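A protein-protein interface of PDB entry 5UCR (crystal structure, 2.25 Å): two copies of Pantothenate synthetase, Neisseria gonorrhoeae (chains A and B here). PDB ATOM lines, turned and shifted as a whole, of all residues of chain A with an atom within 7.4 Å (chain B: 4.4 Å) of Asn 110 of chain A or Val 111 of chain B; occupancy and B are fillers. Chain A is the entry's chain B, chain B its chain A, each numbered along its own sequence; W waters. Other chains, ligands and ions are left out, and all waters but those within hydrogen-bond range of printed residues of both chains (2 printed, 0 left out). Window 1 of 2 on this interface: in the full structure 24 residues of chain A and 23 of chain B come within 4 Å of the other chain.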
ATOM      1  N   LEU A  63      17.261 -12.684  13.104  1.00  0.00           N
ATOM      2  CA  LEU A  63      16.107 -12.947  13.952  1.00  0.00           C
ATOM      3  C   LEU A  63      15.083 -13.888  13.319  1.00  0.00           C
ATOM      4  O   LEU A  63      14.118 -14.259  13.989  1.00  0.00           O
ATOM      5  CB  LEU A  63      15.426 -11.626  14.322  1.00  0.00           C
ATOM      6  CG  LEU A  63      15.721 -10.987  15.680  1.00  0.00           C
ATOM      7  CD1 LEU A  63      17.214 -10.758  15.903  1.00  0.00           C
ATOM      8  CD2 LEU A  63      14.937  -9.683  15.756  1.00  0.00           C
ATOM      9  N   TYR A 102      20.098  -3.486  13.944  1.00  0.00           N
ATOM     10  CA  TYR A 102      20.142  -3.982  15.317  1.00  0.00           C
ATOM     11  C   TYR A 102      21.377  -3.414  16.006  1.00  0.00           C
ATOM     12  O   TYR A 102      22.360  -4.134  16.234  1.00  0.00           O
ATOM     13  CB  TYR A 102      20.141  -5.508  15.347  1.00  0.00           C
ATOM     14  CG  TYR A 102      18.918  -6.087  14.671  1.00  0.00           C
ATOM     15  CD1 TYR A 102      17.669  -6.023  15.275  1.00  0.00           C
ATOM     16  CD2 TYR A 102      19.008  -6.677  13.427  1.00  0.00           C
ATOM     17  CE1 TYR A 102      16.536  -6.550  14.654  1.00  0.00           C
ATOM     18  CE2 TYR A 102      17.896  -7.200  12.801  1.00  0.00           C
ATOM     19  CZ  TYR A 102      16.662  -7.134  13.419  1.00  0.00           C
ATOM     20  OH  TYR A 102      15.556  -7.648  12.792  1.00  0.00           O
ATOM     21  N   GLU A 106      20.468  -7.441  21.264  1.00  0.00           N
ATOM     22  CA  GLU A 106      19.110  -7.927  21.284  1.00  0.00           C
ATOM     23  C   GLU A 106      18.153  -6.957  20.599  1.00  0.00           C
ATOM     24  O   GLU A 106      18.391  -5.745  20.507  1.00  0.00           O
ATOM     25  CB  GLU A 106      18.678  -8.127  22.729  1.00  0.00           C
ATOM     26  CG  GLU A 106      19.046  -6.902  23.563  1.00  0.00           C
ATOM     27  CD  GLU A 106      18.672  -7.024  25.021  1.00  0.00           C
ATOM     28  OE1 GLU A 106      18.175  -8.100  25.421  1.00  0.00           O
ATOM     29  OE2 GLU A 106      18.877  -6.032  25.762  1.00  0.00           O
ATOM     30  N   GLN A 107      17.046  -7.521  20.133  1.00  0.00           N
ATOM     31  CA  GLN A 107      15.849  -6.787  19.743  1.00  0.00           C
ATOM     32  C   GLN A 107      14.869  -6.914  20.907  1.00  0.00           C
ATOM     33  O   GLN A 107      14.245  -7.965  21.102  1.00  0.00           O
ATOM     34  CB  GLN A 107      15.287  -7.355  18.441  1.00  0.00           C
ATOM     35  CG  GLN A 107      13.978  -6.738  17.974  1.00  0.00           C
ATOM     36  CD  GLN A 107      14.162  -5.343  17.417  1.00  0.00           C
ATOM     37  OE1 GLN A 107      15.287  -4.915  17.150  1.00  0.00           O
ATOM     38  NE2 GLN A 107      13.051  -4.615  17.247  1.00  0.00           N
ATOM     39  N   ARG A 108      14.733  -5.838  21.686  1.00  0.00           N
ATOM     40  CA  ARG A 108      13.973  -5.907  22.932  1.00  0.00           C
ATOM     41  C   ARG A 108      12.467  -5.866  22.690  1.00  0.00           C
ATOM     42  O   ARG A 108      11.704  -6.520  23.413  1.00  0.00           O
ATOM     43  CB  ARG A 108      14.369  -4.758  23.865  1.00  0.00           C
ATOM     44  CG  ARG A 108      15.710  -4.861  24.562  1.00  0.00           C
ATOM     45  CD  ARG A 108      16.042  -3.508  25.230  1.00  0.00           C
ATOM     46  NE  ARG A 108      16.025  -2.446  24.221  1.00  0.00           N
ATOM     47  CZ  ARG A 108      16.107  -1.137  24.455  1.00  0.00           C
ATOM     48  NH1 ARG A 108      16.211  -0.667  25.695  1.00  0.00           N
ATOM     49  NH2 ARG A 108      16.075  -0.289  23.427  1.00  0.00           N
ATOM     50  N   TYR A 109      12.025  -5.078  21.711  1.00  0.00           N
ATOM     51  CA  TYR A 109      10.613  -4.878  21.380  1.00  0.00           C
ATOM     52  C   TYR A 109      10.331  -5.594  20.067  1.00  0.00           C
ATOM     53  O   TYR A 109      10.947  -5.281  19.040  1.00  0.00           O
ATOM     54  CB  TYR A 109      10.269  -3.379  21.283  1.00  0.00           C
ATOM     55  CG  TYR A 109      10.348  -2.745  22.646  1.00  0.00           C
ATOM     56  CD1 TYR A 109      11.577  -2.394  23.184  1.00  0.00           C
ATOM     57  CD2 TYR A 109       9.210  -2.567  23.424  1.00  0.00           C
ATOM     58  CE1 TYR A 109      11.678  -1.870  24.459  1.00  0.00           C
ATOM     59  CE2 TYR A 109       9.296  -2.020  24.711  1.00  0.00           C
ATOM     60  CZ  TYR A 109      10.539  -1.689  25.218  1.00  0.00           C
ATOM     61  OH  TYR A 109      10.661  -1.163  26.477  1.00  0.00           O
ATOM     62  N   ASN A 110       9.431  -6.575  20.107  1.00  0.00           N
ATOM     63  CA  ASN A 110       9.172  -7.415  18.952  1.00  0.00           C
ATOM     64  C   ASN A 110       7.698  -7.324  18.603  1.00  0.00           C
ATOM     65  O   ASN A 110       6.861  -7.087  19.468  1.00  0.00           O
ATOM     66  CB  ASN A 110       9.578  -8.873  19.219  1.00  0.00           C
ATOM     67  CG  ASN A 110      11.080  -9.029  19.449  1.00  0.00           C
ATOM     68  OD1 ASN A 110      11.846  -9.228  18.511  1.00  0.00           O
ATOM     69  ND2 ASN A 110      11.508  -8.920  20.716  1.00  0.00           N
ATOM     70  N   VAL A 111       7.378  -7.463  17.324  1.00  0.00           N
ATOM     71  CA  VAL A 111       5.976  -7.558  16.940  1.00  0.00           C
ATOM     72  C   VAL A 111       5.559  -9.016  17.093  1.00  0.00           C
ATOM     73  O   VAL A 111       6.124  -9.902  16.443  1.00  0.00           O
ATOM     74  CB  VAL A 111       5.745  -7.040  15.516  1.00  0.00           C
ATOM     75  CG1 VAL A 111       4.273  -7.168  15.159  1.00  0.00           C
ATOM     76  CG2 VAL A 111       6.196  -5.569  15.411  1.00  0.00           C
ATOM     77  N   GLU A 112       4.594  -9.269  17.974  1.00  0.00           N
ATOM     78  CA  GLU A 112       4.247 -10.637  18.349  1.00  0.00           C
ATOM     79  C   GLU A 112       3.041 -11.110  17.552  1.00  0.00           C
ATOM     80  O   GLU A 112       1.929 -10.612  17.780  1.00  0.00           O
ATOM     81  CB  GLU A 112       3.958 -10.726  19.847  1.00  0.00           C
ATOM     82  CG  GLU A 112       3.830 -12.155  20.371  1.00  0.00           C
ATOM     83  CD  GLU A 112       5.157 -12.890  20.314  1.00  0.00           C
ATOM     84  OE1 GLU A 112       6.208 -12.223  20.389  1.00  0.00           O
ATOM     85  OE2 GLU A 112       5.158 -14.126  20.187  1.00  0.00           O
ATOM     86  N   PRO A 113       3.200 -12.044  16.618  1.00  0.00           N
ATOM     87  CA  PRO A 113       2.037 -12.569  15.879  1.00  0.00           C
ATOM     88  C   PRO A 113       1.130 -13.348  16.809  1.00  0.00           C
ATOM     89  O   PRO A 113       1.533 -13.684  17.936  1.00  0.00           O
ATOM     90  CB  PRO A 113       2.666 -13.496  14.822  1.00  0.00           C
ATOM     91  CG  PRO A 113       4.165 -13.144  14.815  1.00  0.00           C
ATOM     92  CD  PRO A 113       4.458 -12.700  16.226  1.00  0.00           C
ATOM     93  N   ARG A 130       7.674 -14.219  14.171  1.00  0.00           N
ATOM     94  CA  ARG A 130       7.966 -13.072  15.018  1.00  0.00           C
ATOM     95  C   ARG A 130       9.087 -12.224  14.409  1.00  0.00           C
ATOM     96  O   ARG A 130       8.977 -10.997  14.322  1.00  0.00           O
ATOM     97  CB  ARG A 130       8.343 -13.566  16.426  1.00  0.00           C
ATOM     98  CG  ARG A 130       8.750 -12.446  17.396  1.00  0.00           C
ATOM     99  CD  ARG A 130       9.380 -12.975  18.679  1.00  0.00           C
ATOM    100  NE  ARG A 130       8.432 -13.807  19.403  1.00  0.00           N
ATOM    101  CZ  ARG A 130       8.614 -15.103  19.647  1.00  0.00           C
ATOM    102  NH1 ARG A 130       9.726 -15.706  19.249  1.00  0.00           N
ATOM    103  NH2 ARG A 130       7.683 -15.791  20.300  1.00  0.00           N
ATOM    104  N   GLY A 131      10.165 -12.877  13.962  1.00  0.00           N
ATOM    105  CA  GLY A 131      11.271 -12.166  13.327  1.00  0.00           C
ATOM    106  C   GLY A 131      10.887 -11.510  12.009  1.00  0.00           C
ATOM    107  O   GLY A 131      11.351 -10.408  11.690  1.00  0.00           O
ATOM    108  N   ALA A 133       7.751 -10.460  11.291  1.00  0.00           N
ATOM    109  CA  ALA A 133       6.869  -9.334  11.593  1.00  0.00           C
ATOM    110  C   ALA A 133       7.653  -8.151  12.147  1.00  0.00           C
ATOM    111  O   ALA A 133       7.334  -6.991  11.864  1.00  0.00           O
ATOM    112  CB  ALA A 133       5.786  -9.753  12.581  1.00  0.00           C
ATOM    113  N   THR A 134       8.661  -8.431  12.960  1.00  0.00           N
ATOM    114  CA  THR A 134       9.483  -7.375  13.544  1.00  0.00           C
ATOM    115  C   THR A 134      10.336  -6.677  12.491  1.00  0.00           C
ATOM    116  O   THR A 134      10.354  -5.443  12.420  1.00  0.00           O
ATOM    117  CB  THR A 134      10.355  -7.973  14.642  1.00  0.00           C
ATOM    118  OG1 THR A 134       9.490  -8.546  15.613  1.00  0.00           O
ATOM    119  CG2 THR A 134      11.220  -6.912  15.291  1.00  0.00           C
ATOM    120  N   VAL A 135      11.059  -7.441  11.662  1.00  0.00           N
ATOM    121  CA  VAL A 135      11.944  -6.773  10.713  1.00  0.00           C
ATOM    122  C   VAL A 135      11.124  -6.047   9.647  1.00  0.00           C
ATOM    123  O   VAL A 135      11.535  -4.984   9.160  1.00  0.00           O
ATOM    124  CB  VAL A 135      12.977  -7.741  10.097  1.00  0.00           C
ATOM    125  CG1 VAL A 135      12.373  -8.625   8.998  1.00  0.00           C
ATOM    126  CG2 VAL A 135      14.146  -6.952   9.526  1.00  0.00           C
ATOM    127  N   SER A 137       8.121  -4.614  10.120  1.00  0.00           N
ATOM    128  CA  SER A 137       7.715  -3.370  10.777  1.00  0.00           C
ATOM    129  C   SER A 137       8.857  -2.346  10.810  1.00  0.00           C
ATOM    130  O   SER A 137       8.638  -1.155  10.541  1.00  0.00           O
ATOM    131  CB  SER A 137       7.209  -3.678  12.185  1.00  0.00           C
ATOM    132  OG  SER A 137       6.074  -4.550  12.121  1.00  0.00           O
ATOM    133  N   LEU A 168      -1.682  -2.757  13.254  1.00  0.00           N
ATOM    134  CA  LEU A 168      -0.821  -1.664  13.682  1.00  0.00           C
ATOM    135  C   LEU A 168      -1.056  -0.382  12.896  1.00  0.00           C
ATOM    136  O   LEU A 168      -0.343   0.594  13.126  1.00  0.00           O
ATOM    137  CB  LEU A 168       0.655  -2.084  13.583  1.00  0.00           C
ATOM    138  CG  LEU A 168       1.000  -3.295  14.466  1.00  0.00           C
ATOM    139  CD1 LEU A 168       2.465  -3.720  14.296  1.00  0.00           C
ATOM    140  CD2 LEU A 168       0.668  -2.998  15.940  1.00  0.00           C
ATOM    141  N   ASN B 110       0.705  -7.715  18.504  1.00  0.00           N
ATOM    142  CA  ASN B 110       0.969  -6.819  19.614  1.00  0.00           C
ATOM    143  C   ASN B 110       2.455  -6.461  19.647  1.00  0.00           C
ATOM    144  O   ASN B 110       3.315  -7.266  19.275  1.00  0.00           O
ATOM    145  CB  ASN B 110       0.541  -7.466  20.941  1.00  0.00           C
ATOM    146  CG  ASN B 110      -0.957  -7.684  21.029  1.00  0.00           C
ATOM    147  OD1 ASN B 110      -1.696  -6.772  21.403  1.00  0.00           O
ATOM    148  ND2 ASN B 110      -1.416  -8.899  20.700  1.00  0.00           N
ATOM    149  N   VAL B 111       2.757  -5.253  20.089  1.00  0.00           N
ATOM    150  CA  VAL B 111       4.142  -4.892  20.363  1.00  0.00           C
ATOM    151  C   VAL B 111       4.476  -5.432  21.744  1.00  0.00           C
ATOM    152  O   VAL B 111       3.861  -5.039  22.742  1.00  0.00           O
ATOM    153  CB  VAL B 111       4.362  -3.375  20.281  1.00  0.00           C
ATOM    154  CG1 VAL B 111       5.821  -3.013  20.719  1.00  0.00           C
ATOM    155  CG2 VAL B 111       4.098  -2.875  18.860  1.00  0.00           C
ATOM    156  N   GLU B 112       5.419  -6.365  21.793  1.00  0.00           N
ATOM    157  CA  GLU B 112       5.730  -7.107  22.999  1.00  0.00           C
ATOM    158  C   GLU B 112       6.981  -6.509  23.632  1.00  0.00           C
ATOM    159  O   GLU B 112       8.059  -6.578  23.023  1.00  0.00           O
ATOM    160  CB  GLU B 112       5.945  -8.579  22.655  1.00  0.00           C
ATOM    161  CG  GLU B 112       5.983  -9.542  23.828  1.00  0.00           C
ATOM    162  CD  GLU B 112       4.657  -9.636  24.576  1.00  0.00           C
ATOM    163  OE1 GLU B 112       4.677  -9.929  25.795  1.00  0.00           O
ATOM    164  OE2 GLU B 112       3.598  -9.438  23.955  1.00  0.00           O
ATOM    165  N   PRO B 113       6.891  -5.886  24.805  1.00  0.00           N
ATOM    166  CA  PRO B 113       8.087  -5.346  25.452  1.00  0.00           C
ATOM    167  C   PRO B 113       8.956  -6.463  26.003  1.00  0.00           C
ATOM    168  O   PRO B 113       8.542  -7.629  26.038  1.00  0.00           O
ATOM    169  CB  PRO B 113       7.515  -4.479  26.589  1.00  0.00           C
ATOM    170  CG  PRO B 113       6.109  -4.217  26.214  1.00  0.00           C
ATOM    171  CD  PRO B 113       5.661  -5.466  25.500  1.00  0.00           C
ATOM    172  N   ARG B 130       2.269  -4.122  27.511  1.00  0.00           N
ATOM    173  CA  ARG B 130       2.080  -4.595  26.146  1.00  0.00           C
ATOM    174  C   ARG B 130       0.986  -3.790  25.456  1.00  0.00           C
ATOM    175  O   ARG B 130       1.136  -3.392  24.292  1.00  0.00           O
ATOM    176  CB  ARG B 130       1.736  -6.101  26.142  1.00  0.00           C
ATOM    177  CG  ARG B 130       1.094  -6.571  24.848  1.00  0.00           C
ATOM    178  CD  ARG B 130       0.478  -8.004  24.978  1.00  0.00           C
ATOM    179  NE  ARG B 130       1.432  -8.919  25.598  1.00  0.00           N
ATOM    180  CZ  ARG B 130       1.237  -9.589  26.738  1.00  0.00           C
ATOM    181  NH1 ARG B 130       0.089  -9.498  27.409  1.00  0.00           N
ATOM    182  NH2 ARG B 130       2.198 -10.381  27.197  1.00  0.00           N
ATOM    183  N   ALA B 133       2.298  -0.255  24.755  1.00  0.00           N
ATOM    184  CA  ALA B 133       3.237  -0.290  23.641  1.00  0.00           C
ATOM    185  C   ALA B 133       2.500  -0.428  22.318  1.00  0.00           C
ATOM    186  O   ALA B 133       2.844   0.241  21.334  1.00  0.00           O
ATOM    187  CB  ALA B 133       4.229  -1.437  23.827  1.00  0.00           C
ATOM    188  N   THR B 134       1.447  -1.260  22.293  1.00  0.00           N
ATOM    189  CA  THR B 134       0.705  -1.510  21.061  1.00  0.00           C
ATOM    190  C   THR B 134      -0.142  -0.306  20.661  1.00  0.00           C
ATOM    191  O   THR B 134      -0.108   0.125  19.498  1.00  0.00           O
ATOM    192  CB  THR B 134      -0.154  -2.765  21.235  1.00  0.00           C
ATOM    193  OG1 THR B 134       0.705  -3.854  21.575  1.00  0.00           O
ATOM    194  CG2 THR B 134      -0.934  -3.109  19.942  1.00  0.00           C
ATOM    195  N   SER B 137       2.119   2.451  19.339  1.00  0.00           N
ATOM    196  CA  SER B 137       2.585   2.207  17.981  1.00  0.00           C
ATOM    197  C   SER B 137       1.482   2.498  16.967  1.00  0.00           C
ATOM    198  O   SER B 137       1.740   3.117  15.918  1.00  0.00           O
ATOM    199  CB  SER B 137       3.091   0.772  17.842  1.00  0.00           C
ATOM    200  OG  SER B 137       4.107   0.490  18.790  1.00  0.00           O
ATOM    201  N   LEU B 164      10.468   1.031  22.377  1.00  0.00           N
ATOM    202  CA  LEU B 164       9.826   0.632  21.126  1.00  0.00           C
ATOM    203  C   LEU B 164      10.115   1.634  20.014  1.00  0.00           C
ATOM    204  O   LEU B 164      10.130   1.265  18.835  1.00  0.00           O
ATOM    205  CB  LEU B 164       8.308   0.493  21.325  1.00  0.00           C
ATOM    206  CG  LEU B 164       7.442   1.762  21.432  1.00  0.00           C
ATOM    207  CD1 LEU B 164       7.048   2.330  20.043  1.00  0.00           C
ATOM    208  CD2 LEU B 164       6.178   1.514  22.279  1.00  0.00           C
ATOM    209  N   LEU B 168      11.834  -0.315  16.909  1.00  0.00           N
ATOM    210  CA  LEU B 168      11.000  -0.397  15.709  1.00  0.00           C
ATOM    211  C   LEU B 168      11.250   0.764  14.727  1.00  0.00           C
ATOM    212  O   LEU B 168      10.502   0.918  13.753  1.00  0.00           O
ATOM    213  CB  LEU B 168       9.518  -0.456  16.115  1.00  0.00           C
ATOM    214  CG  LEU B 168       9.128  -1.623  17.055  1.00  0.00           C
ATOM    215  CD1 LEU B 168       7.655  -1.610  17.302  1.00  0.00           C
ATOM    216  CD2 LEU B 168       9.529  -2.960  16.445  1.00  0.00           C
HETATM  217  O   HOH W   1       0.397 -11.089  20.043  1.00  0.00           O
HETATM  218  O   HOH W   2       9.479  -8.847  22.784  1.00  0.00           O
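Gln 107 of chain A touches Leu 168 of chain B. O of Arg 108 of chain A touches O of Glu 112 of chain B (3.7 Å). Arg 108 of chain A touches Pro 113 of chain B (O to C, 3.8 Å). Glu 112 of chain B touches Tyr 109 of chain A. Tyr 109 of chain A touches Pro 113 of chain B. Tyr 109 of chain A touches Leu 164 of chain B (CD1 to N, 3.7 Å). Leu 168 of chain B touches Tyr 109 of chain A (CD2 to O, 3.8 Å). Asn 110 of chain B touches Asn 110 of chain A (O to O, 3.6 Å). Asn 110 of chain A touches Val 111 of chain B. Val 111 of chain A touches Asn 110 of chain B.
Asn 110 of chain A touches its own counterpart, Asn 110 of chain B. Asn 110 of chain A touches Val 111 of chain B, and with the chains exchanged Val 111 of chain A touches Asn 110 of chain B. Asn 110 of chain A touches Glu 112 of chain B, and with the chains exchanged Glu 112 of chain A touches Asn 110 of chain B. Positions printed for both chains: 110, 111, 112, 113, 130, 133, 134, 137 and 168.
Of the 17 printed residues of chain A, 6 touch a printed residue of chain B. Hydrophobic or aromatic side chains of chain A within 4 Å of the printed part of chain B: Tyr 109. Of the 10 printed residues of chain B, 6 touch a printed residue of chain A.
The backbone NH (N) of Glu 112 of chain B is in hydrogen-bond range of the backbone carbonyl oxygen (O) of Asn 110 of chain A (2.8 Å). The backbone NH (N) of Glu 112 of chain A sits at hydrogen-bond distance from the backbone carbonyl oxygen (O) of Asn 110 of chain B, 2.7 Å away.
The side-chain carboxylate (OE1) of Glu 112 of chain A is in salt-bridge range of the guanidinium group (NE) of Arg 130 of chain A, 2.9 Å away. NE2 of Gln 107 of chain A is in hydrogen-bond range of O of Tyr 109 of chain A (2.8 Å). OE2 of Glu 112 of chain B lies within salt-bridge range of NE of Arg 130 of chain B. OG1 of Thr 134 of chain A is in hydrogen-bond range of N of Val 111 of chain A, at 2.9 Å. The side-chain hydroxyl (OG1) of Thr 134 of chain B lies within hydrogen-bond range of the backbone NH (N) of Val 111 of chain B. The backbone carbonyl oxygen (O) of Gln 107 of chain A is in hydrogen-bond range of the side-chain amide nitrogen (ND2) of Asn 110 of chain A, 2.9 Å away.
Printed residues of chain B within 4 Å of Arg 108 of chain A: Glu 112 and Pro 113. Asn 110 of chain A touches just these residues of chain B: Asn 110 (3.6 Å), Val 111 (3.6 Å) and Glu 112 (2.8 Å). Printed residues of chain B within 4 Å of Glu 112 of chain A: Asn 110 (2.7 Å). Printed residues of chain A within 4 Å of Asn 110 of chain B: Asn 110, Val 111 and Glu 112. Val 111 of chain B touches one residue of chain A. Of the printed residues of chain A, Glu 112 of chain B touches Arg 108 (3.7 Å), Tyr 109 (3.5 Å) and Asn 110 (2.8 Å). Of the printed residues of chain A, Pro 113 of chain B touches Arg 108 and Tyr 109. The nearest printed residue of chain B that does not touch Glu 112 of chain A is Glu 112 of chain B (4.1 Å).
Water W2 lies within hydrogen-bond range of O of Glu 112 of chain B (2.7 Å), ND2 of Asn 110 of chain A (2.9 Å) and O of Arg 108 of chain A (3.3 Å). Water W1 bridges O of Glu 112 of chain A (2.8 Å) and ND2 of Asn 110 of chain B (2.9 Å).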
